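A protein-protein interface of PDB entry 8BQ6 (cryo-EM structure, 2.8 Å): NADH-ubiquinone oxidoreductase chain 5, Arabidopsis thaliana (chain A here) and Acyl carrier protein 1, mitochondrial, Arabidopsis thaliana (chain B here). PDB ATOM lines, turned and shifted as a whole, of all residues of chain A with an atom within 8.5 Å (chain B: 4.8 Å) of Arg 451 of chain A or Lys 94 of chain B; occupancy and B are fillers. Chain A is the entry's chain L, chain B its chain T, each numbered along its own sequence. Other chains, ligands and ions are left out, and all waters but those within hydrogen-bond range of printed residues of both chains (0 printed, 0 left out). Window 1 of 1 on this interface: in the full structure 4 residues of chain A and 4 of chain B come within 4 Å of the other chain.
The guanidinium group of Arg 451 of chain A is in hydrogen-bond range of the backbone carbonyl oxygen of Ser 121 of chain B (3.2 Å). OD2 of Asp 452 of chain A lies within salt-bridge range of NZ of Lys 94 of chain B (2.7 Å). NZ of Lys 94 of chain B is in salt-bridge range of OE1 of Glu 362 of chain A, at 3.7 Å.
O of Asp 452 of chain A sits at hydrogen-bond distance from SG of Cys 456 of chain A (3.2 Å). The side-chain carboxylate (OD1) of Asp 452 of chain A is in hydrogen-bond range of the side-chain hydroxyl (OG) of Ser 360 of chain A (3.5 Å). The side-chain carboxylate (OD1) of Asp 452 of chain A lies within salt-bridge range of the guanidinium group (NH1) of Arg 451 of chain A (3.97 Å).
Phe 449 of chain A touches Glu 91 of chain B (CE1 to CG, 3.4 Å). Phe 449 of chain A touches Lys 94 of chain B. Arg 451 of chain A touches Phe 93 of chain B (CD to O, 3.7 Å). Arg 451 of chain A touches Lys 94 of chain B (CD to CB, 3.5 Å).
Arg 451 of chain A touches three residues of chain B. Of the printed residues of chain A, Phe 93 of chain B touches Arg 451 (3.7 Å). Lys 94 of chain B touches four residues of chain A. Of the printed residues of chain A, Ser 121 of chain B touches Arg 451 (3.2 Å). The nearest residue of chain B that does not touch Arg 451 of chain A is Met 120 of chain B (4.3 Å). The nearest residue of chain A that does not touch Lys 94 of chain B is Ser 360 of chain A (4.6 Å).
Printed residues of chain A that touch a printed residue of chain B: Glu 362, Phe 449, Arg 451 and Asp 452. Along chain A the printed residues that touch a printed residue of chain B span positions 362 to 452. Among the printed residues, 7 pairs touch across the chains. Among the printed residues, Asp or Glu carboxylates within 4 Å of a Lys or Arg side-chain nitrogen of the other chain: Glu 362 of chain A with Lys 94 of chain B (3.7 Å) and Asp 452 of chain A with Lys 94 of chain B (2.7 Å).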
ATOM      1  N   ILE A 356      13.365   9.890   3.225  1.00  0.00           N
ATOM      2  CA  ILE A 356      14.429   8.972   3.619  1.00  0.00           C
ATOM      3  C   ILE A 356      13.881   7.562   3.797  1.00  0.00           C
ATOM      4  O   ILE A 356      14.465   6.587   3.308  1.00  0.00           O
ATOM      5  CB  ILE A 356      15.116   9.485   4.897  1.00  0.00           C
ATOM      6  CG1 ILE A 356      15.803  10.825   4.631  1.00  0.00           C
ATOM      7  CG2 ILE A 356      16.126   8.485   5.404  1.00  0.00           C
ATOM      8  CD1 ILE A 356      16.044  11.642   5.876  1.00  0.00           C
ATOM      9  N   ALA A 358      11.232   6.423   2.372  1.00  0.00           N
ATOM     10  CA  ALA A 358      10.849   5.972   1.039  1.00  0.00           C
ATOM     11  C   ALA A 358      12.052   5.512   0.231  1.00  0.00           C
ATOM     12  O   ALA A 358      11.955   4.540  -0.526  1.00  0.00           O
ATOM     13  CB  ALA A 358      10.117   7.090   0.299  1.00  0.00           C
ATOM     14  N   MET A 359      13.189   6.189   0.381  1.00  0.00           N
ATOM     15  CA  MET A 359      14.376   5.924  -0.419  1.00  0.00           C
ATOM     16  C   MET A 359      15.353   4.987   0.279  1.00  0.00           C
ATOM     17  O   MET A 359      16.565   5.090   0.065  1.00  0.00           O
ATOM     18  CB  MET A 359      15.063   7.237  -0.783  1.00  0.00           C
ATOM     19  CG  MET A 359      14.259   8.079  -1.748  1.00  0.00           C
ATOM     20  SD  MET A 359      14.235   7.367  -3.402  1.00  0.00           S
ATOM     21  CE  MET A 359      15.957   7.539  -3.849  1.00  0.00           C
ATOM     22  N   SER A 360      14.841   4.078   1.110  1.00  0.00           N
ATOM     23  CA  SER A 360      15.660   3.074   1.791  1.00  0.00           C
ATOM     24  C   SER A 360      16.803   3.719   2.568  1.00  0.00           C
ATOM     25  O   SER A 360      17.973   3.381   2.383  1.00  0.00           O
ATOM     26  CB  SER A 360      16.194   2.037   0.802  1.00  0.00           C
ATOM     27  OG  SER A 360      15.239   1.758  -0.204  1.00  0.00           O
ATOM     28  N   ASP A 361      16.458   4.673   3.431  1.00  0.00           N
ATOM     29  CA  ASP A 361      17.396   5.363   4.310  1.00  0.00           C
ATOM     30  C   ASP A 361      18.541   6.029   3.561  1.00  0.00           C
ATOM     31  O   ASP A 361      19.664   6.093   4.071  1.00  0.00           O
ATOM     32  CB  ASP A 361      17.937   4.420   5.388  1.00  0.00           C
ATOM     33  CG  ASP A 361      16.960   4.238   6.528  1.00  0.00           C
ATOM     34  OD1 ASP A 361      17.222   4.766   7.626  1.00  0.00           O
ATOM     35  OD2 ASP A 361      15.917   3.585   6.321  1.00  0.00           O
ATOM     36  N   GLU A 362      18.273   6.531   2.359  1.00  0.00           N
ATOM     37  CA  GLU A 362      19.212   7.410   1.679  1.00  0.00           C
ATOM     38  C   GLU A 362      19.018   8.836   2.173  1.00  0.00           C
ATOM     39  O   GLU A 362      17.884   9.296   2.341  1.00  0.00           O
ATOM     40  CB  GLU A 362      19.007   7.339   0.166  1.00  0.00           C
ATOM     41  CG  GLU A 362      19.927   8.255  -0.626  1.00  0.00           C
ATOM     42  CD  GLU A 362      21.364   7.780  -0.631  1.00  0.00           C
ATOM     43  OE1 GLU A 362      21.674   6.837  -1.386  1.00  0.00           O
ATOM     44  OE2 GLU A 362      22.182   8.342   0.126  1.00  0.00           O
ATOM     45  N   GLN A 363      20.123   9.538   2.416  1.00  0.00           N
ATOM     46  CA  GLN A 363      20.068  10.898   2.928  1.00  0.00           C
ATOM     47  C   GLN A 363      20.893  11.893   2.132  1.00  0.00           C
ATOM     48  O   GLN A 363      20.787  13.098   2.388  1.00  0.00           O
ATOM     49  CB  GLN A 363      20.535  10.943   4.389  1.00  0.00           C
ATOM     50  CG  GLN A 363      19.469  10.579   5.387  1.00  0.00           C
ATOM     51  CD  GLN A 363      20.050  10.200   6.726  1.00  0.00           C
ATOM     52  OE1 GLN A 363      19.776   9.123   7.252  1.00  0.00           O
ATOM     53  NE2 GLN A 363      20.864  11.083   7.286  1.00  0.00           N
ATOM     54  N   LYS A 367      22.216  11.806  -4.579  1.00  0.00           N
ATOM     55  CA  LYS A 367      21.641  10.570  -5.094  1.00  0.00           C
ATOM     56  C   LYS A 367      20.124  10.596  -4.981  1.00  0.00           C
ATOM     57  O   LYS A 367      19.492   9.604  -4.617  1.00  0.00           O
ATOM     58  CB  LYS A 367      22.216   9.355  -4.373  1.00  0.00           C
ATOM     59  CG  LYS A 367      23.722   9.387  -4.251  1.00  0.00           C
ATOM     60  CD  LYS A 367      24.418   9.234  -5.592  1.00  0.00           C
ATOM     61  CE  LYS A 367      25.925   9.205  -5.394  1.00  0.00           C
ATOM     62  NZ  LYS A 367      26.675   8.496  -6.466  1.00  0.00           N
ATOM     63  N   SER A 448      19.827   9.004  -8.864  1.00  0.00           N
ATOM     64  CA  SER A 448      19.699   8.020  -7.808  1.00  0.00           C
ATOM     65  C   SER A 448      19.929   6.605  -8.340  1.00  0.00           C
ATOM     66  O   SER A 448      20.143   6.384  -9.534  1.00  0.00           O
ATOM     67  CB  SER A 448      18.329   8.170  -7.150  1.00  0.00           C
ATOM     68  OG  SER A 448      17.330   7.475  -7.869  1.00  0.00           O
ATOM     69  N   PHE A 449      19.900   5.635  -7.428  1.00  0.00           N
ATOM     70  CA  PHE A 449      20.089   4.230  -7.763  1.00  0.00           C
ATOM     71  C   PHE A 449      18.756   3.579  -8.105  1.00  0.00           C
ATOM     72  O   PHE A 449      17.720   3.915  -7.525  1.00  0.00           O
ATOM     73  CB  PHE A 449      20.746   3.478  -6.604  1.00  0.00           C
ATOM     74  CG  PHE A 449      22.138   3.934  -6.294  1.00  0.00           C
ATOM     75  CD1 PHE A 449      23.219   3.427  -6.992  1.00  0.00           C
ATOM     76  CD2 PHE A 449      22.370   4.864  -5.299  1.00  0.00           C
ATOM     77  CE1 PHE A 449      24.501   3.843  -6.704  1.00  0.00           C
ATOM     78  CE2 PHE A 449      23.649   5.283  -5.011  1.00  0.00           C
ATOM     79  CZ  PHE A 449      24.716   4.773  -5.715  1.00  0.00           C
ATOM     80  N   GLY A 450      18.794   2.631  -9.043  1.00  0.00           N
ATOM     81  CA  GLY A 450      17.566   2.001  -9.500  1.00  0.00           C
ATOM     82  C   GLY A 450      16.874   1.182  -8.430  1.00  0.00           C
ATOM     83  O   GLY A 450      15.646   1.205  -8.314  1.00  0.00           O
ATOM     84  N   ARG A 451      17.651   0.442  -7.633  1.00  0.00           N
ATOM     85  CA  ARG A 451      17.056  -0.420  -6.617  1.00  0.00           C
ATOM     86  C   ARG A 451      16.287   0.382  -5.575  1.00  0.00           C
ATOM     87  O   ARG A 451      15.336  -0.133  -4.975  1.00  0.00           O
ATOM     88  CB  ARG A 451      18.141  -1.269  -5.957  1.00  0.00           C
ATOM     89  CG  ARG A 451      19.015  -0.524  -4.968  1.00  0.00           C
ATOM     90  CD  ARG A 451      19.936  -1.479  -4.232  1.00  0.00           C
ATOM     91  NE  ARG A 451      19.228  -2.623  -3.672  1.00  0.00           N
ATOM     92  CZ  ARG A 451      18.588  -2.609  -2.511  1.00  0.00           C
ATOM     93  NH1 ARG A 451      18.539  -1.519  -1.762  1.00  0.00           N
ATOM     94  NH2 ARG A 451      17.983  -3.716  -2.091  1.00  0.00           N
ATOM     95  N   ASP A 452      16.677   1.638  -5.345  1.00  0.00           N
ATOM     96  CA  ASP A 452      15.915   2.489  -4.438  1.00  0.00           C
ATOM     97  C   ASP A 452      14.613   2.943  -5.085  1.00  0.00           C
ATOM     98  O   ASP A 452      13.560   2.956  -4.437  1.00  0.00           O
ATOM     99  CB  ASP A 452      16.753   3.699  -4.026  1.00  0.00           C
ATOM    100  CG  ASP A 452      17.943   3.329  -3.154  1.00  0.00           C
ATOM    101  OD1 ASP A 452      17.857   2.343  -2.391  1.00  0.00           O
ATOM    102  OD2 ASP A 452      18.970   4.034  -3.233  1.00  0.00           O
ATOM    103  N   ILE A 453      14.670   3.309  -6.368  1.00  0.00           N
ATOM    104  CA  ILE A 453      13.499   3.828  -7.070  1.00  0.00           C
ATOM    105  C   ILE A 453      12.426   2.756  -7.190  1.00  0.00           C
ATOM    106  O   ILE A 453      11.226   3.034  -7.067  1.00  0.00           O
ATOM    107  CB  ILE A 453      13.915   4.379  -8.446  1.00  0.00           C
ATOM    108  CG1 ILE A 453      14.535   5.767  -8.293  1.00  0.00           C
ATOM    109  CG2 ILE A 453      12.733   4.440  -9.393  1.00  0.00           C
ATOM    110  CD1 ILE A 453      13.705   6.703  -7.456  1.00  0.00           C
ATOM    111  N   SER A 454      12.838   1.514  -7.418  1.00  0.00           N
ATOM    112  CA  SER A 454      11.908   0.405  -7.553  1.00  0.00           C
ATOM    113  C   SER A 454      11.446  -0.161  -6.214  1.00  0.00           C
ATOM    114  O   SER A 454      10.774  -1.197  -6.202  1.00  0.00           O
ATOM    115  CB  SER A 454      12.542  -0.697  -8.403  1.00  0.00           C
ATOM    116  OG  SER A 454      13.933  -0.791  -8.155  1.00  0.00           O
ATOM    117  N   ARG A 455      11.780   0.486  -5.092  1.00  0.00           N
ATOM    118  CA  ARG A 455      11.267   0.080  -3.786  1.00  0.00           C
ATOM    119  C   ARG A 455      10.602   1.244  -3.054  1.00  0.00           C
ATOM    120  O   ARG A 455      10.441   1.188  -1.830  1.00  0.00           O
ATOM    121  CB  ARG A 455      12.378  -0.522  -2.919  1.00  0.00           C
ATOM    122  CG  ARG A 455      11.946  -1.748  -2.115  1.00  0.00           C
ATOM    123  CD  ARG A 455      13.123  -2.459  -1.462  1.00  0.00           C
ATOM    124  NE  ARG A 455      13.628  -1.744  -0.296  1.00  0.00           N
ATOM    125  CZ  ARG A 455      14.895  -1.743   0.092  1.00  0.00           C
ATOM    126  NH1 ARG A 455      15.829  -2.380  -0.595  1.00  0.00           N
ATOM    127  NH2 ARG A 455      15.234  -1.091   1.201  1.00  0.00           N
ATOM    128  N   CYS A 456      10.206   2.288  -3.773  1.00  0.00           N
ATOM    129  CA  CYS A 456       9.649   3.480  -3.153  1.00  0.00           C
ATOM    130  C   CYS A 456       8.209   3.260  -2.694  1.00  0.00           C
ATOM    131  O   CYS A 456       7.457   2.454  -3.250  1.00  0.00           O
ATOM    132  CB  CYS A 456       9.695   4.661  -4.120  1.00  0.00           C
ATOM    133  SG  CYS A 456      11.345   5.218  -4.575  1.00  0.00           S
ATOM    134  N   GLU B  90      28.941  -1.683  -9.626  1.00  0.00           N
ATOM    135  CA  GLU B  90      28.685  -1.105  -8.312  1.00  0.00           C
ATOM    136  C   GLU B  90      27.369  -0.349  -8.277  1.00  0.00           C
ATOM    137  O   GLU B  90      26.539  -0.568  -7.388  1.00  0.00           O
ATOM    138  CB  GLU B  90      29.831  -0.181  -7.923  1.00  0.00           C
ATOM    139  CG  GLU B  90      30.608  -0.705  -6.768  1.00  0.00           C
ATOM    140  CD  GLU B  90      31.946  -0.048  -6.615  1.00  0.00           C
ATOM    141  OE1 GLU B  90      32.902  -0.764  -6.256  1.00  0.00           O
ATOM    142  OE2 GLU B  90      32.046   1.174  -6.841  1.00  0.00           O
ATOM    143  N   GLU B  91      27.159   0.548  -9.238  1.00  0.00           N
ATOM    144  CA  GLU B  91      25.930   1.326  -9.279  1.00  0.00           C
ATOM    145  C   GLU B  91      24.718   0.470  -9.611  1.00  0.00           C
ATOM    146  O   GLU B  91      23.592   0.837  -9.258  1.00  0.00           O
ATOM    147  CB  GLU B  91      26.062   2.448 -10.302  1.00  0.00           C
ATOM    148  CG  GLU B  91      25.102   3.585 -10.084  1.00  0.00           C
ATOM    149  CD  GLU B  91      25.700   4.917 -10.464  1.00  0.00           C
ATOM    150  OE1 GLU B  91      25.036   5.951 -10.250  1.00  0.00           O
ATOM    151  OE2 GLU B  91      26.840   4.929 -10.977  1.00  0.00           O
ATOM    152  N   GLU B  92      24.920  -0.656 -10.294  1.00  0.00           N
ATOM    153  CA  GLU B  92      23.779  -1.464 -10.703  1.00  0.00           C
ATOM    154  C   GLU B  92      23.121  -2.142  -9.510  1.00  0.00           C
ATOM    155  O   GLU B  92      21.889  -2.216  -9.441  1.00  0.00           O
ATOM    156  CB  GLU B  92      24.212  -2.503 -11.735  1.00  0.00           C
ATOM    157  CG  GLU B  92      23.140  -3.528 -12.044  1.00  0.00           C
ATOM    158  CD  GLU B  92      22.009  -2.929 -12.860  1.00  0.00           C
ATOM    159  OE1 GLU B  92      22.196  -1.822 -13.401  1.00  0.00           O
ATOM    160  OE2 GLU B  92      20.936  -3.558 -12.962  1.00  0.00           O
ATOM    161  N   PHE B  93      23.922  -2.635  -8.571  1.00  0.00           N
ATOM    162  CA  PHE B  93      23.427  -3.275  -7.363  1.00  0.00           C
ATOM    163  C   PHE B  93      23.573  -2.389  -6.134  1.00  0.00           C
ATOM    164  O   PHE B  93      23.312  -2.854  -5.020  1.00  0.00           O
ATOM    165  CB  PHE B  93      24.160  -4.601  -7.134  1.00  0.00           C
ATOM    166  CG  PHE B  93      23.939  -5.613  -8.222  1.00  0.00           C
ATOM    167  CD1 PHE B  93      22.797  -6.390  -8.240  1.00  0.00           C
ATOM    168  CD2 PHE B  93      24.881  -5.796  -9.219  1.00  0.00           C
ATOM    169  CE1 PHE B  93      22.594  -7.321  -9.233  1.00  0.00           C
ATOM    170  CE2 PHE B  93      24.678  -6.726 -10.214  1.00  0.00           C
ATOM    171  CZ  PHE B  93      23.534  -7.488 -10.221  1.00  0.00           C
ATOM    172  N   LYS B  94      23.985  -1.133  -6.315  1.00  0.00           N
ATOM    173  CA  LYS B  94      24.201  -0.178  -5.228  1.00  0.00           C
ATOM    174  C   LYS B  94      25.046  -0.788  -4.109  1.00  0.00           C
ATOM    175  O   LYS B  94      24.603  -0.952  -2.971  1.00  0.00           O
ATOM    176  CB  LYS B  94      22.871   0.347  -4.685  1.00  0.00           C
ATOM    177  CG  LYS B  94      23.007   1.634  -3.902  1.00  0.00           C
ATOM    178  CD  LYS B  94      21.783   1.870  -3.056  1.00  0.00           C
ATOM    179  CE  LYS B  94      21.945   3.082  -2.166  1.00  0.00           C
ATOM    180  NZ  LYS B  94      20.735   3.260  -1.324  1.00  0.00           N
ATOM    181  N   LEU B  95      26.279  -1.124  -4.491  1.00  0.00           N
ATOM    182  CA  LEU B  95      27.224  -1.705  -3.513  1.00  0.00           C
ATOM    183  C   LEU B  95      28.439  -0.791  -3.381  1.00  0.00           C
ATOM    184  O   LEU B  95      28.679   0.020  -4.295  1.00  0.00           O
ATOM    185  CB  LEU B  95      27.678  -3.081  -4.011  1.00  0.00           C
ATOM    186  CG  LEU B  95      26.596  -4.145  -4.169  1.00  0.00           C
ATOM    187  CD1 LEU B  95      27.176  -5.409  -4.781  1.00  0.00           C
ATOM    188  CD2 LEU B  95      25.943  -4.455  -2.833  1.00  0.00           C
ATOM    189  N   GLU B  96      29.144  -0.888  -2.263  1.00  0.00           N
ATOM    190  CA  GLU B  96      30.397  -0.170  -2.050  1.00  0.00           C
ATOM    191  C   GLU B  96      31.479  -1.220  -1.829  1.00  0.00           C
ATOM    192  O   GLU B  96      31.738  -1.637  -0.698  1.00  0.00           O
ATOM    193  CB  GLU B  96      30.310   0.807  -0.875  1.00  0.00           C
ATOM    194  CG  GLU B  96      31.510   1.741  -0.798  1.00  0.00           C
ATOM    195  CD  GLU B  96      31.172   3.138  -0.296  1.00  0.00           C
ATOM    196  OE1 GLU B  96      30.138   3.704  -0.707  1.00  0.00           O
ATOM    197  OE2 GLU B  96      31.962   3.680   0.503  1.00  0.00           O
ATOM    198  N   MET B 120      23.401  -7.346   0.305  1.00  0.00           N
ATOM    199  CA  MET B 120      22.804  -5.984   0.210  1.00  0.00           C
ATOM    200  C   MET B 120      22.655  -5.576  -1.262  1.00  0.00           C
ATOM    201  O   MET B 120      22.461  -4.368  -1.519  1.00  0.00           O
ATOM    202  CB  MET B 120      23.678  -4.953   0.933  1.00  0.00           C
ATOM    203  CG  MET B 120      23.757  -5.147   2.434  1.00  0.00           C
ATOM    204  SD  MET B 120      22.135  -5.042   3.226  1.00  0.00           S
ATOM    205  CE  MET B 120      21.752  -3.312   2.951  1.00  0.00           C
ATOM    206  N   SER B 121      22.734  -6.540  -2.184  1.00  0.00           N
ATOM    207  CA  SER B 121      22.631  -6.242  -3.637  1.00  0.00           C
ATOM    208  C   SER B 121      21.168  -5.980  -4.011  1.00  0.00           C
ATOM    209  O   SER B 121      20.946  -5.072  -4.837  1.00  0.00           O
ATOM    210  CB  SER B 121      23.218  -7.358  -4.459  1.00  0.00           C
ATOM    211  OG  SER B 121      24.527  -7.683  -4.020  1.00  0.00           O
